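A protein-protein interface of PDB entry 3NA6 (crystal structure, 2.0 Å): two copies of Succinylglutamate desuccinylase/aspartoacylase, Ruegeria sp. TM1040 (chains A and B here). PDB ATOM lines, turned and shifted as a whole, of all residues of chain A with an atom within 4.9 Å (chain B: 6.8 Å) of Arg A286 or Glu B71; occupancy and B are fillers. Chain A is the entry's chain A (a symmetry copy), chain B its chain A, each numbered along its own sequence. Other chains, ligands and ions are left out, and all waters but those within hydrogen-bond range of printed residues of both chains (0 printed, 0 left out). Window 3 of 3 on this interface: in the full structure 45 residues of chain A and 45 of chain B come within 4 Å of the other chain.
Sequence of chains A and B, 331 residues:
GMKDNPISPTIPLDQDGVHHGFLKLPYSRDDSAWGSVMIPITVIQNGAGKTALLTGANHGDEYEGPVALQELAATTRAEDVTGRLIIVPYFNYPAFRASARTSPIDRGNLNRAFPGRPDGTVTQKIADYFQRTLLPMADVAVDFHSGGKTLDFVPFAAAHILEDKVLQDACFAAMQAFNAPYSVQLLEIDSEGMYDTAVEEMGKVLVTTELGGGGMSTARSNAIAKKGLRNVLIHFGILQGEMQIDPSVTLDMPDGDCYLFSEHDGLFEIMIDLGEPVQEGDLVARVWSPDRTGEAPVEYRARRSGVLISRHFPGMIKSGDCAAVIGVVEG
NH2 of Arg A286 is in salt-bridge range of OE1 of Glu B71 (2.7 Å). The side-chain amino group of Lys B226 is in salt-bridge range of the side-chain carboxylate of Glu A269 (2.7 Å).
The backbone carbonyl oxygen (O) of Glu B71 sits at hydrogen-bond distance from the side-chain hydroxyl (OG1) of Thr B75 (2.7 Å). NZ of Lys B226 is in salt-bridge range of OE1 of Glu B71 (2.7 Å). N of Trp A288 sits at hydrogen-bond distance from O of Leu A267 (2.9 Å). The side-chain carboxylate (OE1) of Glu A269 is in salt-bridge range of the guanidinium group (NH2) of Arg A286. The side-chain carboxylate (OE1) of Glu A269 sits at hydrogen-bond distance from the indole nitrogen (NE1) of Trp A288.
CD2 of Leu A267 touches C of Pro B66, at 3.6 Å. Leu A267 touches Val B67 (CD2 to N, 3.6 Å). CG1 of Val B67 touches CD of Glu A269, 3.5 Å away. NH2 of Arg A286 touches NZ of Lys B226 (3.7 Å). CB of Gln B70 touches CE3 of Trp A288, 3.7 Å away. Trp A288 touches Glu B71. Trp A288 touches Ala B74.
Of the printed residues of chain B, Arg A286 touches Glu B71 and Lys B226. Of the printed residues of chain B, Trp A288 touches Gln B70, Glu B71 and Ala B74. Printed residues of chain A within 4 Å of Pro B66: Leu A267. Printed residues of chain A within 4 Å of Gln B70: Trp A288. Printed residues of chain A within 4 Å of Glu B71: Arg A286 and Trp A288. Leu B72 touches none of the printed residues of chain A. Ala B73 touches none of the printed residues of chain A. Printed residues of chain A within 4 Å of Lys B226: Glu A269 and Arg A286. The nearest printed residue of chain B that does not touch Arg A286 is Thr B75 (5.8 Å).
Of the 13 printed residues of chain A, 4 touch a printed residue of chain B. Hydrophobic or aromatic side chains of chain A within 4 Å of the printed part of chain B: Leu A267 and Trp A288. Of the 13 printed residues of chain B, 6 touch a printed residue of chain A. Among the printed residues, Asp or Glu carboxylates within 4 Å of a Lys or Arg side-chain nitrogen of the other chain: Glu A269 with Lys B226 (2.7 Å) and Arg A286 with Glu B71 (2.7 Å).
No position is printed for both chains. Of the 9 pairs that touch across the chains among the printed residues, none has its exchanged pair printed and touching as well.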
ATOM      1  N   LEU A 267     -30.790 -31.526 -31.816  1.00  0.00           N
ATOM      2  CA  LEU A 267     -30.631 -30.308 -31.039  1.00  0.00           C
ATOM      3  C   LEU A 267     -29.436 -29.535 -31.584  1.00  0.00           C
ATOM      4  O   LEU A 267     -28.309 -30.003 -31.552  1.00  0.00           O
ATOM      5  CB  LEU A 267     -30.400 -30.647 -29.557  1.00  0.00           C
ATOM      6  CG  LEU A 267     -30.202 -29.490 -28.565  1.00  0.00           C
ATOM      7  CD1 LEU A 267     -31.427 -28.609 -28.610  1.00  0.00           C
ATOM      8  CD2 LEU A 267     -29.904 -29.964 -27.122  1.00  0.00           C
ATOM      9  N   PHE A 268     -29.682 -28.319 -32.033  1.00  0.00           N
ATOM     10  CA  PHE A 268     -28.660 -27.544 -32.753  1.00  0.00           C
ATOM     11  C   PHE A 268     -27.902 -26.635 -31.792  1.00  0.00           C
ATOM     12  O   PHE A 268     -28.513 -25.787 -31.114  1.00  0.00           O
ATOM     13  CB  PHE A 268     -29.344 -26.675 -33.793  1.00  0.00           C
ATOM     14  CG  PHE A 268     -28.404 -25.888 -34.646  1.00  0.00           C
ATOM     15  CD1 PHE A 268     -27.530 -26.536 -35.498  1.00  0.00           C
ATOM     16  CD2 PHE A 268     -28.402 -24.515 -34.618  1.00  0.00           C
ATOM     17  CE1 PHE A 268     -26.694 -25.863 -36.313  1.00  0.00           C
ATOM     18  CE2 PHE A 268     -27.509 -23.807 -35.439  1.00  0.00           C
ATOM     19  CZ  PHE A 268     -26.685 -24.502 -36.302  1.00  0.00           C
ATOM     20  N   GLU A 269     -26.592 -26.827 -31.710  1.00  0.00           N
ATOM     21  CA  GLU A 269     -25.746 -25.956 -30.925  1.00  0.00           C
ATOM     22  C   GLU A 269     -24.748 -25.220 -31.822  1.00  0.00           C
ATOM     23  O   GLU A 269     -23.767 -25.813 -32.304  1.00  0.00           O
ATOM     24  CB  GLU A 269     -24.964 -26.701 -29.847  1.00  0.00           C
ATOM     25  CG  GLU A 269     -24.098 -25.700 -29.009  1.00  0.00           C
ATOM     26  CD  GLU A 269     -23.145 -26.359 -28.079  1.00  0.00           C
ATOM     27  OE1 GLU A 269     -23.110 -27.599 -28.081  1.00  0.00           O
ATOM     28  OE2 GLU A 269     -22.414 -25.628 -27.360  1.00  0.00           O
ATOM     29  N   MET A 271     -21.641 -22.632 -32.409  1.00  0.00           N
ATOM     30  CA  MET A 271     -20.458 -22.357 -31.570  1.00  0.00           C
ATOM     31  C   MET A 271     -19.928 -20.920 -31.639  1.00  0.00           C
ATOM     32  O   MET A 271     -19.128 -20.494 -30.794  1.00  0.00           O
ATOM     33  CB  MET A 271     -19.333 -23.324 -31.922  1.00  0.00           C
ATOM     34  CG  MET A 271     -19.735 -24.785 -31.803  1.00  0.00           C
ATOM     35  SD  MET A 271     -20.526 -25.321 -30.068  1.00  0.00           S
ATOM     36  CE  MET A 271     -19.075 -24.933 -28.850  1.00  0.00           C
ATOM     37  N   LEU A 283     -14.672 -25.495 -34.896  1.00  0.00           N
ATOM     38  CA  LEU A 283     -16.026 -25.989 -34.728  1.00  0.00           C
ATOM     39  C   LEU A 283     -16.994 -24.834 -34.967  1.00  0.00           C
ATOM     40  O   LEU A 283     -16.846 -23.786 -34.364  1.00  0.00           O
ATOM     41  CB  LEU A 283     -16.159 -26.531 -33.325  1.00  0.00           C
ATOM     42  CG  LEU A 283     -17.258 -27.495 -32.943  1.00  0.00           C
ATOM     43  CD1 LEU A 283     -17.293 -28.722 -33.834  1.00  0.00           C
ATOM     44  CD2 LEU A 283     -17.000 -27.869 -31.488  1.00  0.00           C
ATOM     45  N   VAL A 284     -17.930 -25.010 -35.891  1.00  0.00           N
ATOM     46  CA  VAL A 284     -18.975 -24.012 -36.164  1.00  0.00           C
ATOM     47  C   VAL A 284     -20.310 -24.399 -35.500  1.00  0.00           C
ATOM     48  O   VAL A 284     -21.067 -23.529 -35.023  1.00  0.00           O
ATOM     49  CB  VAL A 284     -19.168 -23.870 -37.664  1.00  0.00           C
ATOM     50  CG1 VAL A 284     -20.382 -23.031 -38.013  1.00  0.00           C
ATOM     51  CG2 VAL A 284     -17.904 -23.268 -38.248  1.00  0.00           C
ATOM     52  N   ALA A 285     -20.588 -25.695 -35.472  1.00  0.00           N
ATOM     53  CA  ALA A 285     -21.837 -26.193 -34.888  1.00  0.00           C
ATOM     54  C   ALA A 285     -21.720 -27.631 -34.449  1.00  0.00           C
ATOM     55  O   ALA A 285     -20.866 -28.396 -34.975  1.00  0.00           O
ATOM     56  CB  ALA A 285     -22.971 -26.050 -35.873  1.00  0.00           C
ATOM     57  N   ARG A 286     -22.555 -28.013 -33.480  1.00  0.00           N
ATOM     58  CA  ARG A 286     -22.712 -29.417 -33.110  1.00  0.00           C
ATOM     59  C   ARG A 286     -24.186 -29.778 -33.070  1.00  0.00           C
ATOM     60  O   ARG A 286     -25.008 -28.991 -32.582  1.00  0.00           O
ATOM     61  CB  ARG A 286     -22.073 -29.710 -31.756  1.00  0.00           C
ATOM     62  CG  ARG A 286     -20.592 -29.374 -31.702  1.00  0.00           C
ATOM     63  CD  ARG A 286     -19.943 -29.862 -30.421  1.00  0.00           C
ATOM     64  NE  ARG A 286     -20.401 -29.128 -29.251  1.00  0.00           N
ATOM     65  CZ  ARG A 286     -19.972 -29.365 -28.021  1.00  0.00           C
ATOM     66  NH1 ARG A 286     -19.062 -30.322 -27.814  1.00  0.00           N
ATOM     67  NH2 ARG A 286     -20.465 -28.671 -27.002  1.00  0.00           N
ATOM     68  N   VAL A 287     -24.508 -30.964 -33.589  1.00  0.00           N
ATOM     69  CA  VAL A 287     -25.851 -31.522 -33.516  1.00  0.00           C
ATOM     70  C   VAL A 287     -25.932 -32.662 -32.470  1.00  0.00           C
ATOM     71  O   VAL A 287     -25.214 -33.714 -32.583  1.00  0.00           O
ATOM     72  CB  VAL A 287     -26.354 -31.996 -34.895  1.00  0.00           C
ATOM     73  CG1 VAL A 287     -27.841 -32.406 -34.788  1.00  0.00           C
ATOM     74  CG2 VAL A 287     -26.249 -30.843 -35.909  1.00  0.00           C
ATOM     75  N   TRP A 288     -26.761 -32.433 -31.441  1.00  0.00           N
ATOM     76  CA  TRP A 288     -26.922 -33.383 -30.325  1.00  0.00           C
ATOM     77  C   TRP A 288     -28.154 -34.242 -30.614  1.00  0.00           C
ATOM     78  O   TRP A 288     -29.095 -33.798 -31.256  1.00  0.00           O
ATOM     79  CB  TRP A 288     -27.105 -32.659 -28.992  1.00  0.00           C
ATOM     80  CG  TRP A 288     -25.934 -31.865 -28.540  1.00  0.00           C
ATOM     81  CD1 TRP A 288     -25.649 -30.554 -28.838  1.00  0.00           C
ATOM     82  CD2 TRP A 288     -24.856 -32.333 -27.734  1.00  0.00           C
ATOM     83  NE1 TRP A 288     -24.461 -30.181 -28.233  1.00  0.00           N
ATOM     84  CE2 TRP A 288     -23.940 -31.263 -27.579  1.00  0.00           C
ATOM     85  CE3 TRP A 288     -24.570 -33.558 -27.119  1.00  0.00           C
ATOM     86  CZ2 TRP A 288     -22.765 -31.381 -26.821  1.00  0.00           C
ATOM     87  CZ3 TRP A 288     -23.394 -33.682 -26.407  1.00  0.00           C
ATOM     88  CH2 TRP A 288     -22.515 -32.594 -26.251  1.00  0.00           C
ATOM     89  N   PRO A 297     -21.818 -35.789 -29.907  1.00  0.00           N
ATOM     90  CA  PRO A 297     -22.534 -34.961 -30.890  1.00  0.00           C
ATOM     91  C   PRO A 297     -21.876 -35.039 -32.256  1.00  0.00           C
ATOM     92  O   PRO A 297     -20.747 -35.451 -32.331  1.00  0.00           O
ATOM     93  CB  PRO A 297     -22.386 -33.557 -30.324  1.00  0.00           C
ATOM     94  CG  PRO A 297     -21.120 -33.580 -29.516  1.00  0.00           C
ATOM     95  CD  PRO A 297     -20.908 -34.999 -29.052  1.00  0.00           C
ATOM     96  N   VAL A 298     -22.573 -34.675 -33.329  1.00  0.00           N
ATOM     97  CA  VAL A 298     -21.960 -34.597 -34.667  1.00  0.00           C
ATOM     98  C   VAL A 298     -21.455 -33.193 -34.805  1.00  0.00           C
ATOM     99  O   VAL A 298     -22.149 -32.251 -34.451  1.00  0.00           O
ATOM    100  CB  VAL A 298     -22.971 -34.907 -35.791  1.00  0.00           C
ATOM    101  CG1 VAL A 298     -22.329 -34.780 -37.168  1.00  0.00           C
ATOM    102  CG2 VAL A 298     -23.555 -36.324 -35.611  1.00  0.00           C
ATOM    103  N   GLU A 299     -20.255 -33.040 -35.348  1.00  0.00           N
ATOM    104  CA  GLU A 299     -19.594 -31.740 -35.420  1.00  0.00           C
ATOM    105  C   GLU A 299     -19.474 -31.230 -36.836  1.00  0.00           C
ATOM    106  O   GLU A 299     -19.230 -31.999 -37.745  1.00  0.00           O
ATOM    107  CB  GLU A 299     -18.181 -31.871 -34.826  1.00  0.00           C
ATOM    108  CG  GLU A 299     -18.163 -32.283 -33.378  1.00  0.00           C
ATOM    109  CD  GLU A 299     -16.787 -32.227 -32.737  1.00  0.00           C
ATOM    110  OE1 GLU A 299     -15.782 -32.496 -33.422  1.00  0.00           O
ATOM    111  OE2 GLU A 299     -16.730 -31.917 -31.532  1.00  0.00           O
ATOM    112  N   GLY B  65     -30.947 -24.707 -21.831  1.00  0.00           N
ATOM    113  CA  GLY B  65     -30.756 -25.732 -20.810  1.00  0.00           C
ATOM    114  C   GLY B  65     -30.478 -27.084 -21.440  1.00  0.00           C
ATOM    115  O   GLY B  65     -29.516 -27.755 -21.097  1.00  0.00           O
ATOM    116  N   PRO B  66     -31.290 -27.461 -22.422  1.00  0.00           N
ATOM    117  CA  PRO B  66     -31.027 -28.723 -23.096  1.00  0.00           C
ATOM    118  C   PRO B  66     -29.620 -28.874 -23.696  1.00  0.00           C
ATOM    119  O   PRO B  66     -29.027 -29.956 -23.611  1.00  0.00           O
ATOM    120  CB  PRO B  66     -32.111 -28.745 -24.160  1.00  0.00           C
ATOM    121  CG  PRO B  66     -33.272 -28.115 -23.468  1.00  0.00           C
ATOM    122  CD  PRO B  66     -32.650 -26.966 -22.718  1.00  0.00           C
ATOM    123  N   VAL B  67     -29.087 -27.817 -24.303  1.00  0.00           N
ATOM    124  CA  VAL B  67     -27.710 -27.861 -24.812  1.00  0.00           C
ATOM    125  C   VAL B  67     -26.726 -28.093 -23.660  1.00  0.00           C
ATOM    126  O   VAL B  67     -25.850 -28.967 -23.738  1.00  0.00           O
ATOM    127  CB  VAL B  67     -27.368 -26.578 -25.598  1.00  0.00           C
ATOM    128  CG1 VAL B  67     -25.864 -26.524 -25.923  1.00  0.00           C
ATOM    129  CG2 VAL B  67     -28.213 -26.505 -26.875  1.00  0.00           C
ATOM    130  N   ALA B  68     -26.846 -27.293 -22.597  1.00  0.00           N
ATOM    131  CA  ALA B  68     -25.935 -27.396 -21.449  1.00  0.00           C
ATOM    132  C   ALA B  68     -25.996 -28.768 -20.783  1.00  0.00           C
ATOM    133  O   ALA B  68     -24.955 -29.332 -20.374  1.00  0.00           O
ATOM    134  CB  ALA B  68     -26.232 -26.274 -20.416  1.00  0.00           C
ATOM    135  N   LEU B  69     -27.207 -29.330 -20.722  1.00  0.00           N
ATOM    136  CA  LEU B  69     -27.434 -30.617 -20.042  1.00  0.00           C
ATOM    137  C   LEU B  69     -27.017 -31.787 -20.905  1.00  0.00           C
ATOM    138  O   LEU B  69     -26.460 -32.774 -20.373  1.00  0.00           O
ATOM    139  CB  LEU B  69     -28.887 -30.763 -19.541  1.00  0.00           C
ATOM    140  CG  LEU B  69     -29.263 -29.756 -18.434  1.00  0.00           C
ATOM    141  CD1 LEU B  69     -30.778 -29.722 -18.105  1.00  0.00           C
ATOM    142  CD2 LEU B  69     -28.462 -30.101 -17.150  1.00  0.00           C
ATOM    143  N   GLN B  70     -27.227 -31.701 -22.223  1.00  0.00           N
ATOM    144  CA  GLN B  70     -26.728 -32.780 -23.071  1.00  0.00           C
ATOM    145  C   GLN B  70     -25.203 -32.833 -22.965  1.00  0.00           C
ATOM    146  O   GLN B  70     -24.638 -33.913 -22.855  1.00  0.00           O
ATOM    147  CB  GLN B  70     -27.126 -32.646 -24.542  1.00  0.00           C
ATOM    148  CG  GLN B  70     -28.531 -33.076 -24.862  1.00  0.00           C
ATOM    149  CD  GLN B  70     -28.690 -34.619 -24.857  1.00  0.00           C
ATOM    150  OE1 GLN B  70     -28.285 -35.311 -23.914  1.00  0.00           O
ATOM    151  NE2 GLN B  70     -29.293 -35.136 -25.887  1.00  0.00           N
ATOM    152  N   GLU B  71     -24.543 -31.676 -22.979  1.00  0.00           N
ATOM    153  CA  GLU B  71     -23.073 -31.665 -22.886  1.00  0.00           C
ATOM    154  C   GLU B  71     -22.617 -32.195 -21.524  1.00  0.00           C
ATOM    155  O   GLU B  71     -21.711 -33.013 -21.434  1.00  0.00           O
ATOM    156  CB  GLU B  71     -22.522 -30.275 -23.108  1.00  0.00           C
ATOM    157  CG  GLU B  71     -21.012 -30.237 -23.163  1.00  0.00           C
ATOM    158  CD  GLU B  71     -20.476 -28.841 -23.216  1.00  0.00           C
ATOM    159  OE1 GLU B  71     -20.462 -28.232 -24.306  1.00  0.00           O
ATOM    160  OE2 GLU B  71     -20.054 -28.353 -22.164  1.00  0.00           O
ATOM    161  N   LEU B  72     -23.278 -31.752 -20.467  1.00  0.00           N
ATOM    162  CA  LEU B  72     -22.978 -32.257 -19.131  1.00  0.00           C
ATOM    163  C   LEU B  72     -23.093 -33.785 -19.074  1.00  0.00           C
ATOM    164  O   LEU B  72     -22.197 -34.452 -18.571  1.00  0.00           O
ATOM    165  CB  LEU B  72     -23.897 -31.621 -18.066  1.00  0.00           C
ATOM    166  CG  LEU B  72     -23.422 -31.860 -16.615  1.00  0.00           C
ATOM    167  CD1 LEU B  72     -22.196 -30.988 -16.282  1.00  0.00           C
ATOM    168  CD2 LEU B  72     -24.538 -31.618 -15.646  1.00  0.00           C
ATOM    169  N   ALA B  73     -24.157 -34.331 -19.637  1.00  0.00           N
ATOM    170  CA  ALA B  73     -24.399 -35.782 -19.523  1.00  0.00           C
ATOM    171  C   ALA B  73     -23.360 -36.570 -20.332  1.00  0.00           C
ATOM    172  O   ALA B  73     -22.982 -37.687 -19.960  1.00  0.00           O
ATOM    173  CB  ALA B  73     -25.799 -36.143 -19.986  1.00  0.00           C
ATOM    174  N   ALA B  74     -22.901 -35.977 -21.419  1.00  0.00           N
ATOM    175  CA  ALA B  74     -22.007 -36.667 -22.352  1.00  0.00           C
ATOM    176  C   ALA B  74     -20.539 -36.514 -21.995  1.00  0.00           C
ATOM    177  O   ALA B  74     -19.733 -37.270 -22.473  1.00  0.00           O
ATOM    178  CB  ALA B  74     -22.238 -36.145 -23.775  1.00  0.00           C
ATOM    179  N   THR B  75     -20.177 -35.520 -21.200  1.00  0.00           N
ATOM    180  CA  THR B  75     -18.761 -35.198 -21.009  1.00  0.00           C
ATOM    181  C   THR B  75     -18.271 -35.256 -19.544  1.00  0.00           C
ATOM    182  O   THR B  75     -17.121 -35.033 -19.290  1.00  0.00           O
ATOM    183  CB  THR B  75     -18.421 -33.808 -21.632  1.00  0.00           C
ATOM    184  OG1 THR B  75     -19.032 -32.768 -20.872  1.00  0.00           O
ATOM    185  CG2 THR B  75     -18.898 -33.716 -23.085  1.00  0.00           C
ATOM    186  N   THR B  76     -19.123 -35.576 -18.578  1.00  0.00           N
ATOM    187  CA  THR B  76     -18.715 -35.541 -17.172  1.00  0.00           C
ATOM    188  C   THR B  76     -18.326 -36.949 -16.785  1.00  0.00           C
ATOM    189  O   THR B  76     -19.097 -37.882 -17.052  1.00  0.00           O
ATOM    190  CB  THR B  76     -19.881 -35.112 -16.292  1.00  0.00           C
ATOM    191  OG1 THR B  76     -20.314 -33.805 -16.702  1.00  0.00           O
ATOM    192  CG2 THR B  76     -19.493 -35.120 -14.800  1.00  0.00           C
ATOM    193  N   LYS B 226     -24.080 -23.023 -19.586  1.00  0.00           N
ATOM    194  CA  LYS B 226     -23.019 -23.932 -19.183  1.00  0.00           C
ATOM    195  C   LYS B 226     -22.228 -23.434 -17.951  1.00  0.00           C
ATOM    196  O   LYS B 226     -21.902 -24.238 -17.039  1.00  0.00           O
ATOM    197  CB  LYS B 226     -22.039 -24.192 -20.331  1.00  0.00           C
ATOM    198  CG  LYS B 226     -22.638 -24.969 -21.496  1.00  0.00           C
ATOM    199  CD  LYS B 226     -21.605 -25.174 -22.613  1.00  0.00           C
ATOM    200  CE  LYS B 226     -22.255 -25.631 -23.913  1.00  0.00           C
ATOM    201  NZ  LYS B 226     -21.257 -25.716 -24.976  1.00  0.00           N
